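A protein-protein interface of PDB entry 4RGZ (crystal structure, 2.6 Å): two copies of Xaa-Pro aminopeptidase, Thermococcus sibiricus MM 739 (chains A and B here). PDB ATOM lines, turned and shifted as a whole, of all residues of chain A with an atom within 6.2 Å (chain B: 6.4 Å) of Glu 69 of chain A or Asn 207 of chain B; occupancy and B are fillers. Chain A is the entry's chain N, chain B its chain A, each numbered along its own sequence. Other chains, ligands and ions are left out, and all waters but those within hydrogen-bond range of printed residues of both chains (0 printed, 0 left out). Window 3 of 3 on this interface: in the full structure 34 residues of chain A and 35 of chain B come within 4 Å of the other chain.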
ATOM      1  N   PHE A  38      26.906  17.346  -1.139  1.00  0.00           N
ATOM      2  CA  PHE A  38      26.618  18.748  -1.350  1.00  0.00           C
ATOM      3  C   PHE A  38      27.867  19.457  -1.877  1.00  0.00           C
ATOM      4  O   PHE A  38      28.949  19.322  -1.301  1.00  0.00           O
ATOM      5  CB  PHE A  38      26.199  19.415  -0.033  1.00  0.00           C
ATOM      6  CG  PHE A  38      24.725  19.314   0.300  1.00  0.00           C
ATOM      7  CD1 PHE A  38      23.787  20.152  -0.315  1.00  0.00           C
ATOM      8  CD2 PHE A  38      24.275  18.438   1.302  1.00  0.00           C
ATOM      9  CE1 PHE A  38      22.434  20.090   0.032  1.00  0.00           C
ATOM     10  CE2 PHE A  38      22.921  18.368   1.654  1.00  0.00           C
ATOM     11  CZ  PHE A  38      22.000  19.196   1.017  1.00  0.00           C
ATOM     12  N   LEU A  65      21.222  32.237   3.112  1.00  0.00           N
ATOM     13  CA  LEU A  65      20.648  32.205   1.762  1.00  0.00           C
ATOM     14  C   LEU A  65      20.834  30.871   1.047  1.00  0.00           C
ATOM     15  O   LEU A  65      20.482  30.722  -0.128  1.00  0.00           O
ATOM     16  CB  LEU A  65      21.213  33.340   0.896  1.00  0.00           C
ATOM     17  CG  LEU A  65      22.038  34.499   1.480  1.00  0.00           C
ATOM     18  CD1 LEU A  65      22.647  35.305   0.339  1.00  0.00           C
ATOM     19  CD2 LEU A  65      21.258  35.397   2.440  1.00  0.00           C
ATOM     20  N   TYR A  66      21.377  29.898   1.768  1.00  0.00           N
ATOM     21  CA  TYR A  66      21.654  28.602   1.201  1.00  0.00           C
ATOM     22  C   TYR A  66      20.626  27.535   1.553  1.00  0.00           C
ATOM     23  O   TYR A  66      20.640  26.464   0.952  1.00  0.00           O
ATOM     24  CB  TYR A  66      23.049  28.147   1.622  1.00  0.00           C
ATOM     25  CG  TYR A  66      24.143  28.633   0.698  1.00  0.00           C
ATOM     26  CD1 TYR A  66      24.415  27.969  -0.501  1.00  0.00           C
ATOM     27  CD2 TYR A  66      24.913  29.757   1.020  1.00  0.00           C
ATOM     28  CE1 TYR A  66      25.413  28.415  -1.354  1.00  0.00           C
ATOM     29  CE2 TYR A  66      25.923  30.199   0.174  1.00  0.00           C
ATOM     30  CZ  TYR A  66      26.166  29.526  -1.011  1.00  0.00           C
ATOM     31  OH  TYR A  66      27.154  29.961  -1.854  1.00  0.00           O
ATOM     32  N   GLU A  67      19.727  27.825   2.499  1.00  0.00           N
ATOM     33  CA  GLU A  67      18.868  26.768   3.068  1.00  0.00           C
ATOM     34  C   GLU A  67      17.898  26.104   2.088  1.00  0.00           C
ATOM     35  O   GLU A  67      17.755  24.885   2.101  1.00  0.00           O
ATOM     36  CB  GLU A  67      18.107  27.231   4.316  1.00  0.00           C
ATOM     37  CG  GLU A  67      17.556  26.065   5.146  1.00  0.00           C
ATOM     38  CD  GLU A  67      16.396  26.448   6.059  1.00  0.00           C
ATOM     39  OE1 GLU A  67      16.101  27.659   6.202  1.00  0.00           O
ATOM     40  OE2 GLU A  67      15.776  25.526   6.641  1.00  0.00           O
ATOM     41  N   LYS A  68      17.233  26.896   1.249  1.00  0.00           N
ATOM     42  CA  LYS A  68      16.254  26.341   0.305  1.00  0.00           C
ATOM     43  C   LYS A  68      16.876  25.511  -0.834  1.00  0.00           C
ATOM     44  O   LYS A  68      16.167  25.057  -1.735  1.00  0.00           O
ATOM     45  CB  LYS A  68      15.297  27.427  -0.214  1.00  0.00           C
ATOM     46  CG  LYS A  68      14.288  27.918   0.827  1.00  0.00           C
ATOM     47  CD  LYS A  68      12.957  28.273   0.193  1.00  0.00           C
ATOM     48  CE  LYS A  68      12.108  29.098   1.145  1.00  0.00           C
ATOM     49  NZ  LYS A  68      10.722  29.317   0.645  1.00  0.00           N
ATOM     50  N   GLU A  69      18.204  25.344  -0.780  1.00  0.00           N
ATOM     51  CA  GLU A  69      18.942  24.268  -1.469  1.00  0.00           C
ATOM     52  C   GLU A  69      19.741  23.461  -0.415  1.00  0.00           C
ATOM     53  O   GLU A  69      20.907  23.095  -0.607  1.00  0.00           O
ATOM     54  CB  GLU A  69      19.828  24.800  -2.616  1.00  0.00           C
ATOM     55  CG  GLU A  69      19.101  24.936  -3.959  1.00  0.00           C
ATOM     56  CD  GLU A  69      20.010  25.049  -5.194  1.00  0.00           C
ATOM     57  OE1 GLU A  69      19.472  25.460  -6.250  1.00  0.00           O
ATOM     58  OE2 GLU A  69      21.229  24.726  -5.141  1.00  0.00           O
ATOM     59  N   LEU A  70      19.063  23.219   0.707  1.00  0.00           N
ATOM     60  CA  LEU A  70      19.532  22.411   1.829  1.00  0.00           C
ATOM     61  C   LEU A  70      18.294  21.784   2.471  1.00  0.00           C
ATOM     62  O   LEU A  70      18.184  21.705   3.699  1.00  0.00           O
ATOM     63  CB  LEU A  70      20.230  23.287   2.869  1.00  0.00           C
ATOM     64  CG  LEU A  70      21.715  23.589   2.782  1.00  0.00           C
ATOM     65  CD1 LEU A  70      22.057  24.652   3.811  1.00  0.00           C
ATOM     66  CD2 LEU A  70      22.520  22.327   3.024  1.00  0.00           C
ATOM     67  N   GLU A  71      17.362  21.358   1.620  1.00  0.00           N
ATOM     68  CA  GLU A  71      16.073  20.801   2.032  1.00  0.00           C
ATOM     69  C   GLU A  71      16.209  19.641   3.037  1.00  0.00           C
ATOM     70  O   GLU A  71      15.410  19.535   3.987  1.00  0.00           O
ATOM     71  CB  GLU A  71      15.277  20.356   0.796  1.00  0.00           C
ATOM     72  CG  GLU A  71      13.768  20.244   1.013  1.00  0.00           C
ATOM     73  CD  GLU A  71      12.979  21.401   0.422  1.00  0.00           C
ATOM     74  OE1 GLU A  71      11.737  21.401   0.568  1.00  0.00           O
ATOM     75  OE2 GLU A  71      13.590  22.300  -0.196  1.00  0.00           O
ATOM     76  N   ILE B 198      25.597  32.227 -14.220  1.00  0.00           N
ATOM     77  CA  ILE B 198      24.336  31.753 -13.669  1.00  0.00           C
ATOM     78  C   ILE B 198      23.167  32.129 -14.576  1.00  0.00           C
ATOM     79  O   ILE B 198      22.934  33.303 -14.906  1.00  0.00           O
ATOM     80  CB  ILE B 198      24.053  32.405 -12.313  1.00  0.00           C
ATOM     81  CG1 ILE B 198      25.163  32.111 -11.293  1.00  0.00           C
ATOM     82  CG2 ILE B 198      22.711  31.951 -11.783  1.00  0.00           C
ATOM     83  CD1 ILE B 198      25.282  33.213 -10.218  1.00  0.00           C
ATOM     84  N   ALA B 200      19.048  31.414 -14.592  1.00  0.00           N
ATOM     85  CA  ALA B 200      17.962  30.896 -13.772  1.00  0.00           C
ATOM     86  C   ALA B 200      16.616  31.285 -14.395  1.00  0.00           C
ATOM     87  O   ALA B 200      16.271  32.489 -14.449  1.00  0.00           O
ATOM     88  CB  ALA B 200      18.095  31.408 -12.337  1.00  0.00           C
ATOM     89  N   PRO B 203      10.709  29.344 -12.421  1.00  0.00           N
ATOM     90  CA  PRO B 203      10.746  29.221 -10.939  1.00  0.00           C
ATOM     91  C   PRO B 203      12.171  29.158 -10.379  1.00  0.00           C
ATOM     92  O   PRO B 203      12.403  29.563  -9.240  1.00  0.00           O
ATOM     93  CB  PRO B 203       9.993  27.918 -10.668  1.00  0.00           C
ATOM     94  CG  PRO B 203       9.181  27.668 -11.903  1.00  0.00           C
ATOM     95  CD  PRO B 203       9.995  28.205 -13.044  1.00  0.00           C
ATOM     96  N   ASN B 204      13.125  28.691 -11.191  1.00  0.00           N
ATOM     97  CA  ASN B 204      14.534  28.648 -10.774  1.00  0.00           C
ATOM     98  C   ASN B 204      15.124  30.008 -10.492  1.00  0.00           C
ATOM     99  O   ASN B 204      16.063  30.127  -9.676  1.00  0.00           O
ATOM    100  CB  ASN B 204      15.401  27.894 -11.768  1.00  0.00           C
ATOM    101  CG  ASN B 204      15.152  26.424 -11.709  1.00  0.00           C
ATOM    102  OD1 ASN B 204      15.222  25.726 -12.711  1.00  0.00           O
ATOM    103  ND2 ASN B 204      14.816  25.936 -10.518  1.00  0.00           N
ATOM    104  N   GLY B 205      14.576  31.039 -11.130  1.00  0.00           N
ATOM    105  CA  GLY B 205      15.019  32.397 -10.819  1.00  0.00           C
ATOM    106  C   GLY B 205      14.809  32.870  -9.397  1.00  0.00           C
ATOM    107  O   GLY B 205      15.362  33.888  -8.996  1.00  0.00           O
ATOM    108  N   ALA B 206      13.995  32.145  -8.637  1.00  0.00           N
ATOM    109  CA  ALA B 206      13.509  32.601  -7.330  1.00  0.00           C
ATOM    110  C   ALA B 206      14.543  32.321  -6.296  1.00  0.00           C
ATOM    111  O   ALA B 206      14.436  32.766  -5.164  1.00  0.00           O
ATOM    112  CB  ALA B 206      12.204  31.889  -6.959  1.00  0.00           C
ATOM    113  N   ASN B 207      15.532  31.538  -6.687  1.00  0.00           N
ATOM    114  CA  ASN B 207      16.574  31.107  -5.791  1.00  0.00           C
ATOM    115  C   ASN B 207      17.901  31.759  -6.191  1.00  0.00           C
ATOM    116  O   ASN B 207      18.502  31.380  -7.194  1.00  0.00           O
ATOM    117  CB  ASN B 207      16.640  29.568  -5.798  1.00  0.00           C
ATOM    118  CG  ASN B 207      17.621  29.012  -4.777  1.00  0.00           C
ATOM    119  OD1 ASN B 207      17.631  27.806  -4.513  1.00  0.00           O
ATOM    120  ND2 ASN B 207      18.463  29.882  -4.201  1.00  0.00           N
ATOM    121  N   PRO B 208      18.367  32.748  -5.401  1.00  0.00           N
ATOM    122  CA  PRO B 208      19.552  33.519  -5.822  1.00  0.00           C
ATOM    123  C   PRO B 208      20.776  32.645  -6.026  1.00  0.00           C
ATOM    124  O   PRO B 208      21.699  33.062  -6.724  1.00  0.00           O
ATOM    125  CB  PRO B 208      19.783  34.473  -4.652  1.00  0.00           C
ATOM    126  CG  PRO B 208      18.439  34.609  -4.017  1.00  0.00           C
ATOM    127  CD  PRO B 208      17.875  33.214  -4.089  1.00  0.00           C
ATOM    128  N   HIS B 209      20.754  31.437  -5.446  1.00  0.00           N
ATOM    129  CA  HIS B 209      21.925  30.558  -5.387  1.00  0.00           C
ATOM    130  C   HIS B 209      21.917  29.445  -6.427  1.00  0.00           C
ATOM    131  O   HIS B 209      22.674  28.474  -6.339  1.00  0.00           O
ATOM    132  CB  HIS B 209      22.043  30.004  -3.967  1.00  0.00           C
ATOM    133  CG  HIS B 209      22.586  31.012  -2.952  1.00  0.00           C
ATOM    134  ND1 HIS B 209      22.732  32.336  -3.227  1.00  0.00           N
ATOM    135  CD2 HIS B 209      23.004  30.845  -1.626  1.00  0.00           C
ATOM    136  CE1 HIS B 209      23.215  32.977  -2.135  1.00  0.00           C
ATOM    137  NE2 HIS B 209      23.386  32.066  -1.160  1.00  0.00           N
ATOM    138  N   HIS B 210      21.087  29.605  -7.451  1.00  0.00           N
ATOM    139  CA  HIS B 210      20.739  28.539  -8.331  1.00  0.00           C
ATOM    140  C   HIS B 210      21.867  28.080  -9.194  1.00  0.00           C
ATOM    141  O   HIS B 210      22.593  28.865  -9.739  1.00  0.00           O
ATOM    142  CB  HIS B 210      19.544  28.975  -9.182  1.00  0.00           C
ATOM    143  CG  HIS B 210      19.095  27.944 -10.183  1.00  0.00           C
ATOM    144  ND1 HIS B 210      18.528  26.785  -9.820  1.00  0.00           N
ATOM    145  CD2 HIS B 210      19.149  27.940 -11.567  1.00  0.00           C
ATOM    146  CE1 HIS B 210      18.243  26.070 -10.916  1.00  0.00           C
ATOM    147  NE2 HIS B 210      18.627  26.776 -11.984  1.00  0.00           N
ATOM    148  N   ARG B 211      21.982  26.773  -9.351  1.00  0.00           N
ATOM    149  CA  ARG B 211      22.955  26.167 -10.223  1.00  0.00           C
ATOM    150  C   ARG B 211      22.197  25.817 -11.511  1.00  0.00           C
ATOM    151  O   ARG B 211      21.244  25.043 -11.468  1.00  0.00           O
ATOM    152  CB  ARG B 211      23.516  24.907  -9.532  1.00  0.00           C
ATOM    153  CG  ARG B 211      24.636  24.145 -10.232  1.00  0.00           C
ATOM    154  CD  ARG B 211      24.693  22.714  -9.666  1.00  0.00           C
ATOM    155  NE  ARG B 211      25.489  21.748 -10.451  1.00  0.00           N
ATOM    156  CZ  ARG B 211      25.339  20.413 -10.423  1.00  0.00           C
ATOM    157  NH1 ARG B 211      24.407  19.835  -9.661  1.00  0.00           N
ATOM    158  NH2 ARG B 211      26.127  19.638 -11.170  1.00  0.00           N
ATOM    159  N   ILE B 296      16.347  38.820  -0.475  1.00  0.00           N
ATOM    160  CA  ILE B 296      16.975  37.981   0.550  1.00  0.00           C
ATOM    161  C   ILE B 296      18.481  38.069   0.607  1.00  0.00           C
ATOM    162  O   ILE B 296      19.153  37.134   1.007  1.00  0.00           O
ATOM    163  CB  ILE B 296      16.462  36.546   0.474  1.00  0.00           C
ATOM    164  CG1 ILE B 296      16.587  35.998  -0.960  1.00  0.00           C
ATOM    165  CG2 ILE B 296      15.014  36.551   0.906  1.00  0.00           C
ATOM    166  CD1 ILE B 296      15.871  34.662  -1.178  1.00  0.00           C
ATOM    167  N   TYR B 334      12.490  37.826  -5.160  1.00  0.00           N
ATOM    168  CA  TYR B 334      12.470  36.377  -5.356  1.00  0.00           C
ATOM    169  C   TYR B 334      11.204  35.767  -4.812  1.00  0.00           C
ATOM    170  O   TYR B 334      10.958  35.770  -3.597  1.00  0.00           O
ATOM    171  CB  TYR B 334      13.684  35.742  -4.717  1.00  0.00           C
ATOM    172  CG  TYR B 334      14.927  36.436  -5.183  1.00  0.00           C
ATOM    173  CD1 TYR B 334      15.532  36.098  -6.419  1.00  0.00           C
ATOM    174  CD2 TYR B 334      15.462  37.500  -4.441  1.00  0.00           C
ATOM    175  CE1 TYR B 334      16.652  36.761  -6.855  1.00  0.00           C
ATOM    176  CE2 TYR B 334      16.588  38.165  -4.869  1.00  0.00           C
ATOM    177  CZ  TYR B 334      17.193  37.788  -6.067  1.00  0.00           C
ATOM    178  OH  TYR B 334      18.330  38.486  -6.488  1.00  0.00           O
ATOM    179  N   LEU B 335      10.434  35.224  -5.742  1.00  0.00           N
ATOM    180  CA  LEU B 335       9.102  34.788  -5.472  1.00  0.00           C
ATOM    181  C   LEU B 335       9.007  33.298  -5.692  1.00  0.00           C
ATOM    182  O   LEU B 335       8.880  32.814  -6.829  1.00  0.00           O
ATOM    183  CB  LEU B 335       8.087  35.567  -6.326  1.00  0.00           C
ATOM    184  CG  LEU B 335       7.960  37.080  -6.042  1.00  0.00           C
ATOM    185  CD1 LEU B 335       6.788  37.650  -6.829  1.00  0.00           C
ATOM    186  CD2 LEU B 335       7.801  37.439  -4.575  1.00  0.00           C
ATOM    187  N   GLN B 336       9.074  32.573  -4.581  1.00  0.00           N
ATOM    188  CA  GLN B 336       9.111  31.126  -4.623  1.00  0.00           C
ATOM    189  C   GLN B 336       7.979  30.572  -5.486  1.00  0.00           C
ATOM    190  O   GLN B 336       6.838  31.000  -5.376  1.00  0.00           O
ATOM    191  CB  GLN B 336       9.091  30.557  -3.210  1.00  0.00           C
ATOM    192  CG  GLN B 336       9.822  29.229  -3.080  1.00  0.00           C
ATOM    193  CD  GLN B 336      11.326  29.361  -3.308  1.00  0.00           C
ATOM    194  OE1 GLN B 336      11.931  30.399  -3.003  1.00  0.00           O
ATOM    195  NE2 GLN B 336      11.941  28.298  -3.841  1.00  0.00           N
ATOM    196  N   GLY B 340      12.113  35.218 -10.417  1.00  0.00           N
ATOM    197  CA  GLY B 340      12.902  36.224  -9.705  1.00  0.00           C
ATOM    198  C   GLY B 340      13.251  37.371 -10.639  1.00  0.00           C
ATOM    199  O   GLY B 340      13.181  37.204 -11.869  1.00  0.00           O
ATOM    200  N   ARG B 342      16.580  40.281 -10.695  1.00  0.00           N
ATOM    201  CA  ARG B 342      17.752  40.991 -10.182  1.00  0.00           C
ATOM    202  C   ARG B 342      18.353  41.835 -11.312  1.00  0.00           C
ATOM    203  O   ARG B 342      18.415  41.398 -12.457  1.00  0.00           O
ATOM    204  CB  ARG B 342      18.794  40.023  -9.611  1.00  0.00           C
ATOM    205  CG  ARG B 342      20.026  40.711  -8.985  1.00  0.00           C
ATOM    206  CD  ARG B 342      21.248  39.805  -8.857  1.00  0.00           C
ATOM    207  NE  ARG B 342      20.768  38.540  -8.369  1.00  0.00           N
ATOM    208  CZ  ARG B 342      20.880  37.350  -8.943  1.00  0.00           C
ATOM    209  NH1 ARG B 342      21.606  37.145 -10.034  1.00  0.00           N
ATOM    210  NH2 ARG B 342      20.274  36.344  -8.346  1.00  0.00           N
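Of the 8 printed residues of chain A, 4 touch a printed residue of chain B. Hydrophobic or aromatic side chains of chain A within 4 Å of the printed part of chain B: Leu 65 and Tyr 66. Of the 17 printed residues of chain B, 5 touch a printed residue of chain A. Hydrophobic or aromatic side chains of chain B that line the printed part of chain A: His 209 and His 210. Among the printed residues, 6 pairs touch across the chains. Among the printed residues, no Asp or Glu carboxylate lies within 4 Å of a Lys or Arg side-chain nitrogen of the other chain.
Among the printed residues, merely in contact across the chains: Leu 65 of chain A with Ile 296 of chain B (3.1 Å), Tyr 66 of chain A with His 209 of chain B (3.4 Å), Lys 68 of chain A with Gln 336 of chain B (3.8 Å) and Glu 69 of chain A with His 210 of chain B (3.9 Å).
Of the printed residues of chain B, Lys 68 of chain A touches Gln 336 (3.8 Å). Glu 69 of chain A touches two residues of chain B. Asn 207 of chain B touches just one residue of chain A: Glu 69. Printed residues of chain A within 4 Å of His 210 of chain B: Glu 69 (3.9 Å). Printed residues of chain A within 4 Å of Gln 336 of chain B: Lys 68. The nearest residue of chain A that does not touch Asn 207 of chain B is Lys 68 of chain A (4.2 Å).
The side-chain amide nitrogen of Asn 207 of chain B lies close to the backbone NH of His 209 of chain B (3.0 Å).
No position is printed for both chains. Of the 6 pairs that touch across the chains among the printed residues, none has its exchanged pair printed and touching as well.
OD1 of Asn 207 of chain B sits close to OE1 of Glu 69 of chain A. The backbone carbonyl oxygen of Leu 65 of chain A sits close to a ring nitrogen (NE2) of His 209 of chain B, 3.4 Å away.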
